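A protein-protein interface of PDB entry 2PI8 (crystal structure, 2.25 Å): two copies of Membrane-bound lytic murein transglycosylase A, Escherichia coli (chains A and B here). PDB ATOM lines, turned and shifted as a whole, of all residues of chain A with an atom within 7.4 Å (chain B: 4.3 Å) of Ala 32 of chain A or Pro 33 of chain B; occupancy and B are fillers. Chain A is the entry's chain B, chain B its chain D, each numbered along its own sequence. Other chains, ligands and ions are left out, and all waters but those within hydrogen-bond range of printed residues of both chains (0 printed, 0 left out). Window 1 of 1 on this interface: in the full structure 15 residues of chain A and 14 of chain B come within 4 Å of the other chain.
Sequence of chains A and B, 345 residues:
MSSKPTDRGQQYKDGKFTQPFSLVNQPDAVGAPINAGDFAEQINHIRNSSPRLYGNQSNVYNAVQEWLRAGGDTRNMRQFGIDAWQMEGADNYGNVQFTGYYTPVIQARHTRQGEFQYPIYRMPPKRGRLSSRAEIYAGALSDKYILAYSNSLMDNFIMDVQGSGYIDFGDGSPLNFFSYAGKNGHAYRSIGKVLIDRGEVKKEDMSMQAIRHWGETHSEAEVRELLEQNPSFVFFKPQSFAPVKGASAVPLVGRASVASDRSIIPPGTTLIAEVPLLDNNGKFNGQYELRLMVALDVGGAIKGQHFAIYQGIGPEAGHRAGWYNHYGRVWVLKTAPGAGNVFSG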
ATOM      1  N   ALA A  29     -32.653 -15.064  11.348  1.00  0.00           N
ATOM      2  CA  ALA A  29     -31.825 -16.263  11.371  1.00  0.00           C
ATOM      3  C   ALA A  29     -32.369 -17.354  10.457  1.00  0.00           C
ATOM      4  O   ALA A  29     -33.579 -17.468  10.260  1.00  0.00           O
ATOM      5  CB  ALA A  29     -31.714 -16.783  12.794  1.00  0.00           C
ATOM      6  N   VAL A  30     -31.461 -18.158   9.908  1.00  0.00           N
ATOM      7  CA  VAL A  30     -31.829 -19.253   9.016  1.00  0.00           C
ATOM      8  C   VAL A  30     -32.234 -20.518   9.771  1.00  0.00           C
ATOM      9  O   VAL A  30     -32.885 -21.401   9.208  1.00  0.00           O
ATOM     10  CB  VAL A  30     -30.685 -19.591   8.028  1.00  0.00           C
ATOM     11  CG1 VAL A  30     -30.545 -18.487   6.992  1.00  0.00           C
ATOM     12  CG2 VAL A  30     -29.368 -19.790   8.779  1.00  0.00           C
ATOM     13  N   GLY A  31     -31.855 -20.598  11.046  1.00  0.00           N
ATOM     14  CA  GLY A  31     -32.192 -21.762  11.846  1.00  0.00           C
ATOM     15  C   GLY A  31     -31.826 -21.627  13.311  1.00  0.00           C
ATOM     16  O   GLY A  31     -32.473 -20.887  14.052  1.00  0.00           O
ATOM     17  N   ALA A  32     -30.784 -22.343  13.727  1.00  0.00           N
ATOM     18  CA  ALA A  32     -30.324 -22.318  15.115  1.00  0.00           C
ATOM     19  C   ALA A  32     -28.795 -22.286  15.198  1.00  0.00           C
ATOM     20  O   ALA A  32     -28.107 -22.670  14.251  1.00  0.00           O
ATOM     21  CB  ALA A  32     -30.869 -23.534  15.865  1.00  0.00           C
ATOM     22  N   PRO A  33     -28.247 -21.797  16.329  1.00  0.00           N
ATOM     23  CA  PRO A  33     -26.799 -21.707  16.551  1.00  0.00           C
ATOM     24  C   PRO A  33     -26.096 -23.055  16.402  1.00  0.00           C
ATOM     25  O   PRO A  33     -26.344 -23.988  17.171  1.00  0.00           O
ATOM     26  CB  PRO A  33     -26.713 -21.186  17.984  1.00  0.00           C
ATOM     27  CG  PRO A  33     -27.917 -20.311  18.083  1.00  0.00           C
ATOM     28  CD  PRO A  33     -28.979 -21.173  17.446  1.00  0.00           C
ATOM     29  N   ILE A  34     -25.216 -23.144  15.407  1.00  0.00           N
ATOM     30  CA  ILE A  34     -24.476 -24.373  15.133  1.00  0.00           C
ATOM     31  C   ILE A  34     -23.244 -24.540  16.022  1.00  0.00           C
ATOM     32  O   ILE A  34     -22.549 -25.555  15.948  1.00  0.00           O
ATOM     33  CB  ILE A  34     -24.022 -24.448  13.654  1.00  0.00           C
ATOM     34  CG1 ILE A  34     -22.837 -23.513  13.410  1.00  0.00           C
ATOM     35  CG2 ILE A  34     -25.173 -24.071  12.727  1.00  0.00           C
ATOM     36  CD1 ILE A  34     -22.001 -23.912  12.225  1.00  0.00           C
ATOM     37  N   ASN A  35     -22.967 -23.531  16.843  1.00  0.00           N
ATOM     38  CA  ASN A  35     -21.816 -23.567  17.738  1.00  0.00           C
ATOM     39  C   ASN A  35     -22.217 -23.432  19.205  1.00  0.00           C
ATOM     40  O   ASN A  35     -21.633 -22.643  19.951  1.00  0.00           O
ATOM     41  CB  ASN A  35     -20.806 -22.479  17.352  1.00  0.00           C
ATOM     42  CG  ASN A  35     -21.355 -21.073  17.522  1.00  0.00           C
ATOM     43  OD1 ASN A  35     -22.567 -20.860  17.558  1.00  0.00           O
ATOM     44  ND2 ASN A  35     -20.457 -20.104  17.633  1.00  0.00           N
ATOM     45  N   ALA A  36     -23.215 -24.212  19.614  1.00  0.00           N
ATOM     46  CA  ALA A  36     -23.694 -24.189  20.993  1.00  0.00           C
ATOM     47  C   ALA A  36     -22.575 -24.597  21.947  1.00  0.00           C
ATOM     48  O   ALA A  36     -22.369 -23.961  22.983  1.00  0.00           O
ATOM     49  CB  ALA A  36     -24.889 -25.119  21.148  1.00  0.00           C
ATOM     50  N   TRP A  67     -31.226 -20.273  26.650  1.00  0.00           N
ATOM     51  CA  TRP A  67     -31.964 -20.178  25.396  1.00  0.00           C
ATOM     52  C   TRP A  67     -31.475 -21.296  24.479  1.00  0.00           C
ATOM     53  O   TRP A  67     -32.273 -21.976  23.832  1.00  0.00           O
ATOM     54  CB  TRP A  67     -31.726 -18.811  24.746  1.00  0.00           C
ATOM     55  CG  TRP A  67     -32.100 -18.752  23.296  1.00  0.00           C
ATOM     56  CD1 TRP A  67     -33.262 -19.191  22.729  1.00  0.00           C
ATOM     57  CD2 TRP A  67     -31.291 -18.257  22.221  1.00  0.00           C
ATOM     58  NE1 TRP A  67     -33.224 -19.005  21.369  1.00  0.00           N
ATOM     59  CE2 TRP A  67     -32.028 -18.434  21.029  1.00  0.00           C
ATOM     60  CE3 TRP A  67     -30.015 -17.682  22.148  1.00  0.00           C
ATOM     61  CZ2 TRP A  67     -31.530 -18.056  19.776  1.00  0.00           C
ATOM     62  CZ3 TRP A  67     -29.519 -17.306  20.901  1.00  0.00           C
ATOM     63  CH2 TRP A  67     -30.278 -17.497  19.733  1.00  0.00           C
ATOM     64  N   LEU A  68     -30.155 -21.474  24.435  1.00  0.00           N
ATOM     65  CA  LEU A  68     -29.529 -22.517  23.628  1.00  0.00           C
ATOM     66  C   LEU A  68     -29.991 -23.883  24.118  1.00  0.00           C
ATOM     67  O   LEU A  68     -30.089 -24.834  23.341  1.00  0.00           O
ATOM     68  CB  LEU A  68     -28.003 -22.423  23.725  1.00  0.00           C
ATOM     69  CG  LEU A  68     -27.264 -21.720  22.585  1.00  0.00           C
ATOM     70  CD1 LEU A  68     -27.921 -20.395  22.261  1.00  0.00           C
ATOM     71  CD2 LEU A  68     -25.802 -21.529  22.957  1.00  0.00           C
ATOM     72  N   GLY A  71     -33.222 -25.534  22.828  1.00  0.00           N
ATOM     73  CA  GLY A  71     -33.135 -25.933  21.434  1.00  0.00           C
ATOM     74  C   GLY A  71     -32.623 -24.825  20.532  1.00  0.00           C
ATOM     75  O   GLY A  71     -32.553 -24.998  19.314  1.00  0.00           O
ATOM     76  N   GLY A  72     -32.258 -23.693  21.132  1.00  0.00           N
ATOM     77  CA  GLY A  72     -31.755 -22.560  20.372  1.00  0.00           C
ATOM     78  C   GLY A  72     -32.803 -21.987  19.437  1.00  0.00           C
ATOM     79  O   GLY A  72     -32.524 -21.736  18.263  1.00  0.00           O
ATOM     80  N   ASP A  73     -34.008 -21.782  19.960  1.00  0.00           N
ATOM     81  CA  ASP A  73     -35.113 -21.248  19.171  1.00  0.00           C
ATOM     82  C   ASP A  73     -35.007 -19.732  19.031  1.00  0.00           C
ATOM     83  O   ASP A  73     -35.370 -18.983  19.941  1.00  0.00           O
ATOM     84  CB  ASP A  73     -36.451 -21.635  19.809  1.00  0.00           C
ATOM     85  CG  ASP A  73     -37.550 -21.842  18.782  1.00  0.00           C
ATOM     86  OD1 ASP A  73     -37.968 -20.856  18.141  1.00  0.00           O
ATOM     87  OD2 ASP A  73     -37.994 -22.997  18.615  1.00  0.00           O
ATOM     88  N   THR A  74     -34.521 -19.293  17.872  1.00  0.00           N
ATOM     89  CA  THR A  74     -34.336 -17.874  17.566  1.00  0.00           C
ATOM     90  C   THR A  74     -35.608 -17.034  17.694  1.00  0.00           C
ATOM     91  O   THR A  74     -35.547 -15.803  17.697  1.00  0.00           O
ATOM     92  CB  THR A  74     -33.745 -17.689  16.146  1.00  0.00           C
ATOM     93  OG1 THR A  74     -33.528 -16.298  15.888  1.00  0.00           O
ATOM     94  CG2 THR A  74     -34.686 -18.258  15.089  1.00  0.00           C
ATOM     95  N   ILE A 272     -24.561 -12.489  17.672  1.00  0.00           N
ATOM     96  CA  ILE A 272     -25.113 -13.572  16.863  1.00  0.00           C
ATOM     97  C   ILE A 272     -25.051 -13.041  15.432  1.00  0.00           C
ATOM     98  O   ILE A 272     -25.552 -11.953  15.146  1.00  0.00           O
ATOM     99  CB  ILE A 272     -26.571 -13.937  17.268  1.00  0.00           C
ATOM    100  CG1 ILE A 272     -27.095 -15.074  16.386  1.00  0.00           C
ATOM    101  CG2 ILE A 272     -27.482 -12.728  17.188  1.00  0.00           C
ATOM    102  CD1 ILE A 272     -28.504 -15.519  16.724  1.00  0.00           C
ATOM    103  N   GLU A 274     -24.807 -13.830  10.891  1.00  0.00           N
ATOM    104  CA  GLU A 274     -25.023 -14.637   9.701  1.00  0.00           C
ATOM    105  C   GLU A 274     -23.740 -14.575   8.882  1.00  0.00           C
ATOM    106  O   GLU A 274     -23.582 -13.721   8.008  1.00  0.00           O
ATOM    107  CB  GLU A 274     -26.198 -14.085   8.889  1.00  0.00           C
ATOM    108  CG  GLU A 274     -27.561 -14.540   9.377  1.00  0.00           C
ATOM    109  CD  GLU A 274     -27.873 -15.970   8.981  1.00  0.00           C
ATOM    110  OE1 GLU A 274     -27.580 -16.891   9.772  1.00  0.00           O
ATOM    111  OE2 GLU A 274     -28.411 -16.175   7.874  1.00  0.00           O
ATOM    112  N   GLU A 289     -24.412 -18.773   7.573  1.00  0.00           N
ATOM    113  CA  GLU A 289     -24.224 -19.647   8.725  1.00  0.00           C
ATOM    114  C   GLU A 289     -24.461 -18.873  10.018  1.00  0.00           C
ATOM    115  O   GLU A 289     -23.836 -17.841  10.256  1.00  0.00           O
ATOM    116  CB  GLU A 289     -22.802 -20.210   8.701  1.00  0.00           C
ATOM    117  CG  GLU A 289     -22.484 -21.225   9.778  1.00  0.00           C
ATOM    118  CD  GLU A 289     -21.106 -21.832   9.599  1.00  0.00           C
ATOM    119  OE1 GLU A 289     -20.105 -21.095   9.722  1.00  0.00           O
ATOM    120  OE2 GLU A 289     -21.022 -23.047   9.323  1.00  0.00           O
ATOM    121  N   LEU A 290     -25.369 -19.378  10.851  1.00  0.00           N
ATOM    122  CA  LEU A 290     -25.694 -18.728  12.117  1.00  0.00           C
ATOM    123  C   LEU A 290     -24.734 -19.139  13.234  1.00  0.00           C
ATOM    124  O   LEU A 290     -24.653 -20.314  13.597  1.00  0.00           O
ATOM    125  CB  LEU A 290     -27.137 -19.044  12.520  1.00  0.00           C
ATOM    126  CG  LEU A 290     -27.722 -18.175  13.636  1.00  0.00           C
ATOM    127  CD1 LEU A 290     -27.784 -16.721  13.182  1.00  0.00           C
ATOM    128  CD2 LEU A 290     -29.106 -18.678  14.010  1.00  0.00           C
ATOM    129  N   ARG A 291     -24.022 -18.157  13.781  1.00  0.00           N
ATOM    130  CA  ARG A 291     -23.057 -18.402  14.850  1.00  0.00           C
ATOM    131  C   ARG A 291     -23.103 -17.372  15.970  1.00  0.00           C
ATOM    132  O   ARG A 291     -23.376 -16.194  15.739  1.00  0.00           O
ATOM    133  CB  ARG A 291     -21.629 -18.435  14.293  1.00  0.00           C
ATOM    134  CG  ARG A 291     -21.254 -19.694  13.543  1.00  0.00           C
ATOM    135  CD  ARG A 291     -19.792 -19.649  13.129  1.00  0.00           C
ATOM    136  NE  ARG A 291     -19.374 -20.880  12.463  1.00  0.00           N
ATOM    137  CZ  ARG A 291     -18.981 -21.982  13.094  1.00  0.00           C
ATOM    138  NH1 ARG A 291     -18.942 -22.017  14.420  1.00  0.00           N
ATOM    139  NH2 ARG A 291     -18.639 -23.056  12.396  1.00  0.00           N
ATOM    140  N   GLY B  31     -37.699 -25.258  13.632  1.00  0.00           N
ATOM    141  CA  GLY B  31     -36.337 -24.757  13.599  1.00  0.00           C
ATOM    142  C   GLY B  31     -35.291 -25.804  13.261  1.00  0.00           C
ATOM    143  O   GLY B  31     -35.608 -26.972  13.026  1.00  0.00           O
ATOM    144  N   ALA B  32     -34.034 -25.370  13.238  1.00  0.00           N
ATOM    145  CA  ALA B  32     -32.903 -26.240  12.927  1.00  0.00           C
ATOM    146  C   ALA B  32     -32.339 -26.912  14.180  1.00  0.00           C
ATOM    147  O   ALA B  32     -32.588 -26.461  15.300  1.00  0.00           O
ATOM    148  CB  ALA B  32     -31.813 -25.434  12.230  1.00  0.00           C
ATOM    149  N   PRO B  33     -31.599 -28.024  14.005  1.00  0.00           N
ATOM    150  CA  PRO B  33     -30.995 -28.758  15.124  1.00  0.00           C
ATOM    151  C   PRO B  33     -30.012 -27.874  15.892  1.00  0.00           C
ATOM    152  O   PRO B  33     -29.368 -26.998  15.310  1.00  0.00           O
ATOM    153  CB  PRO B  33     -30.272 -29.905  14.422  1.00  0.00           C
ATOM    154  CG  PRO B  33     -31.136 -30.162  13.234  1.00  0.00           C
ATOM    155  CD  PRO B  33     -31.407 -28.763  12.744  1.00  0.00           C
ATOM    156  N   ILE B  34     -29.895 -28.112  17.193  1.00  0.00           N
ATOM    157  CA  ILE B  34     -29.001 -27.325  18.035  1.00  0.00           C
ATOM    158  C   ILE B  34     -27.515 -27.628  17.798  1.00  0.00           C
ATOM    159  O   ILE B  34     -26.677 -26.727  17.870  1.00  0.00           O
ATOM    160  CB  ILE B  34     -29.362 -27.490  19.540  1.00  0.00           C
ATOM    161  CG1 ILE B  34     -28.601 -26.471  20.393  1.00  0.00           C
ATOM    162  CG2 ILE B  34     -29.070 -28.907  20.008  1.00  0.00           C
ATOM    163  CD1 ILE B  34     -28.923 -25.024  20.062  1.00  0.00           C
ATOM    164  N   ASN B  35     -27.200 -28.884  17.483  1.00  0.00           N
ATOM    165  CA  ASN B  35     -25.815 -29.289  17.245  1.00  0.00           C
ATOM    166  C   ASN B  35     -25.493 -29.585  15.776  1.00  0.00           C
ATOM    167  O   ASN B  35     -25.149 -30.712  15.417  1.00  0.00           O
ATOM    168  CB  ASN B  35     -25.448 -30.490  18.132  1.00  0.00           C
ATOM    169  CG  ASN B  35     -26.282 -31.727  17.834  1.00  0.00           C
ATOM    170  OD1 ASN B  35     -27.318 -31.652  17.171  1.00  0.00           O
ATOM    171  ND2 ASN B  35     -25.824 -32.877  18.318  1.00  0.00           N
ATOM    172  N   ALA B  36     -25.583 -28.560  14.933  1.00  0.00           N
ATOM    173  CA  ALA B  36     -25.300 -28.707  13.509  1.00  0.00           C
ATOM    174  C   ALA B  36     -23.799 -28.773  13.239  1.00  0.00           C
ATOM    175  O   ALA B  36     -23.311 -29.731  12.641  1.00  0.00           O
ATOM    176  CB  ALA B  36     -25.929 -27.569  12.727  1.00  0.00           C
ATOM    177  N   TRP B  67     -28.316 -29.806   4.089  1.00  0.00           N
ATOM    178  CA  TRP B  67     -29.612 -29.564   4.715  1.00  0.00           C
ATOM    179  C   TRP B  67     -29.446 -28.627   5.914  1.00  0.00           C
ATOM    180  O   TRP B  67     -30.285 -27.759   6.157  1.00  0.00           O
ATOM    181  CB  TRP B  67     -30.229 -30.902   5.150  1.00  0.00           C
ATOM    182  CG  TRP B  67     -31.412 -30.788   6.070  1.00  0.00           C
ATOM    183  CD1 TRP B  67     -32.594 -30.151   5.820  1.00  0.00           C
ATOM    184  CD2 TRP B  67     -31.516 -31.318   7.398  1.00  0.00           C
ATOM    185  NE1 TRP B  67     -33.426 -30.247   6.909  1.00  0.00           N
ATOM    186  CE2 TRP B  67     -32.789 -30.958   7.892  1.00  0.00           C
ATOM    187  CE3 TRP B  67     -30.656 -32.060   8.218  1.00  0.00           C
ATOM    188  CZ2 TRP B  67     -33.223 -31.314   9.174  1.00  0.00           C
ATOM    189  CZ3 TRP B  67     -31.089 -32.415   9.494  1.00  0.00           C
ATOM    190  CH2 TRP B  67     -32.362 -32.040   9.957  1.00  0.00           C
ATOM    191  N   LEU B  68     -28.344 -28.799   6.641  1.00  0.00           N
ATOM    192  CA  LEU B  68     -28.036 -27.983   7.811  1.00  0.00           C
ATOM    193  C   LEU B  68     -27.521 -26.602   7.417  1.00  0.00           C
ATOM    194  O   LEU B  68     -27.838 -25.604   8.068  1.00  0.00           O
ATOM    195  CB  LEU B  68     -26.988 -28.683   8.682  1.00  0.00           C
ATOM    196  CG  LEU B  68     -27.384 -30.003   9.345  1.00  0.00           C
ATOM    197  CD1 LEU B  68     -26.162 -30.663   9.963  1.00  0.00           C
ATOM    198  CD2 LEU B  68     -28.454 -29.754  10.391  1.00  0.00           C
ATOM    199  N   GLY B  72     -31.953 -26.177   7.881  1.00  0.00           N
ATOM    200  CA  GLY B  72     -31.956 -27.080   9.018  1.00  0.00           C
ATOM    201  C   GLY B  72     -33.333 -27.484   9.512  1.00  0.00           C
ATOM    202  O   GLY B  72     -33.446 -28.343  10.385  1.00  0.00           O
ATOM    203  N   LEU B 290     -33.771 -30.684  19.585  1.00  0.00           N
ATOM    204  CA  LEU B 290     -33.468 -31.355  18.325  1.00  0.00           C
ATOM    205  C   LEU B 290     -31.966 -31.570  18.148  1.00  0.00           C
ATOM    206  O   LEU B 290     -31.196 -30.611  18.064  1.00  0.00           O
ATOM    207  CB  LEU B 290     -34.031 -30.553  17.149  1.00  0.00           C
ATOM    208  CG  LEU B 290     -34.092 -31.283  15.805  1.00  0.00           C
ATOM    209  CD1 LEU B 290     -34.951 -32.534  15.931  1.00  0.00           C
ATOM    210  CD2 LEU B 290     -34.655 -30.354  14.743  1.00  0.00           C
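Ala 32 of chain A touches Pro 33 of chain B, but with the chains exchanged Pro 33 of chain A does not touch Ala 32 of chain B (6.5 Å).
Pro 33 of chain A touches Ile 34 of chain B, but with the chains exchanged Ile 34 of chain A does not touch Pro 33 of chain B (5.6 Å).
Leu 68 of chain A touches Ile 34 of chain B, but with the chains exchanged Ile 34 of chain A does not touch Leu 68 of chain B (5.6 Å).
Gly 72 of chain A touches Ile 34 of chain B, but with the chains exchanged Ile 34 of chain A does not touch Gly 72 of chain B (8.3 Å).
10 positions are printed for both chains.
Printed residues of chain B that touch a printed residue of chain A: Ala 32, Pro 33, Ile 34 and Ala 36.
Hydrophobic or aromatic side chains of chain B within 4 Å of the printed part of chain A: Ala 32, Ile 34 and Ala 36.
Of the 19 printed residues of chain A, 7 touch a printed residue of chain B.
Printed residues of chain A that touch a printed residue of chain B: Gly 31, Ala 32, Pro 33, Ile 34, Leu 68, Gly 71 and Gly 72.
Among the printed residues, 8 pairs touch across the chains.
The backbone NH (N) of Ile 34 of chain B sits at hydrogen-bond distance from the backbone carbonyl oxygen (O) of Leu 290 of chain B.
The backbone carbonyl oxygen of Trp 67 of chain A is in hydrogen-bond range of the backbone NH of Gly 72 of chain A, 3.2 Å away.
N of Ile 34 of chain A is in hydrogen-bond range of O of Leu 290 of chain A.
CA of Gly 31 of chain A touches CB of Ala 32 of chain B, 3.7 Å away.
Ala 32 of chain B touches Ala 32 of chain A.
Ala 32 of chain A touches Pro 33 of chain B (CB to O, 3.8 Å).
CB of Ala 36 of chain B touches CG2 of Ile 34 of chain A, at 3.6 Å.
Ile 34 of chain B touches Leu 68 of chain A.
Gly 71 of chain A touches Ile 34 of chain B (O to CD1, 3.7 Å).
Ile 34 of chain B touches Gly 72 of chain A (CD1 to N, 3.7 Å).
O of Pro 33 of chain A sits close to O of Ile 34 of chain B, 2.8 Å away.
Of chain B, only Ala 32 (3.4 Å) and Pro 33 (3.8 Å) come within 4 Å of Ala 32 of chain A.
Pro 33 of chain B touches just one residue of chain A: Ala 32.
Of the printed residues of chain B, Ile 34 of chain A touches Ala 36.
Printed residues of chain B within 4 Å of Leu 68 of chain A: Ile 34 (3.5 Å).
Glu 274 of chain A touches none of the printed residues of chain B.
The nearest printed residue of chain B that does not touch Ala 32 of chain A is Ile 34 of chain B (4.8 Å).
The nearest residue of chain A that does not touch Pro 33 of chain B is Pro 33 of chain A (4.7 Å).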
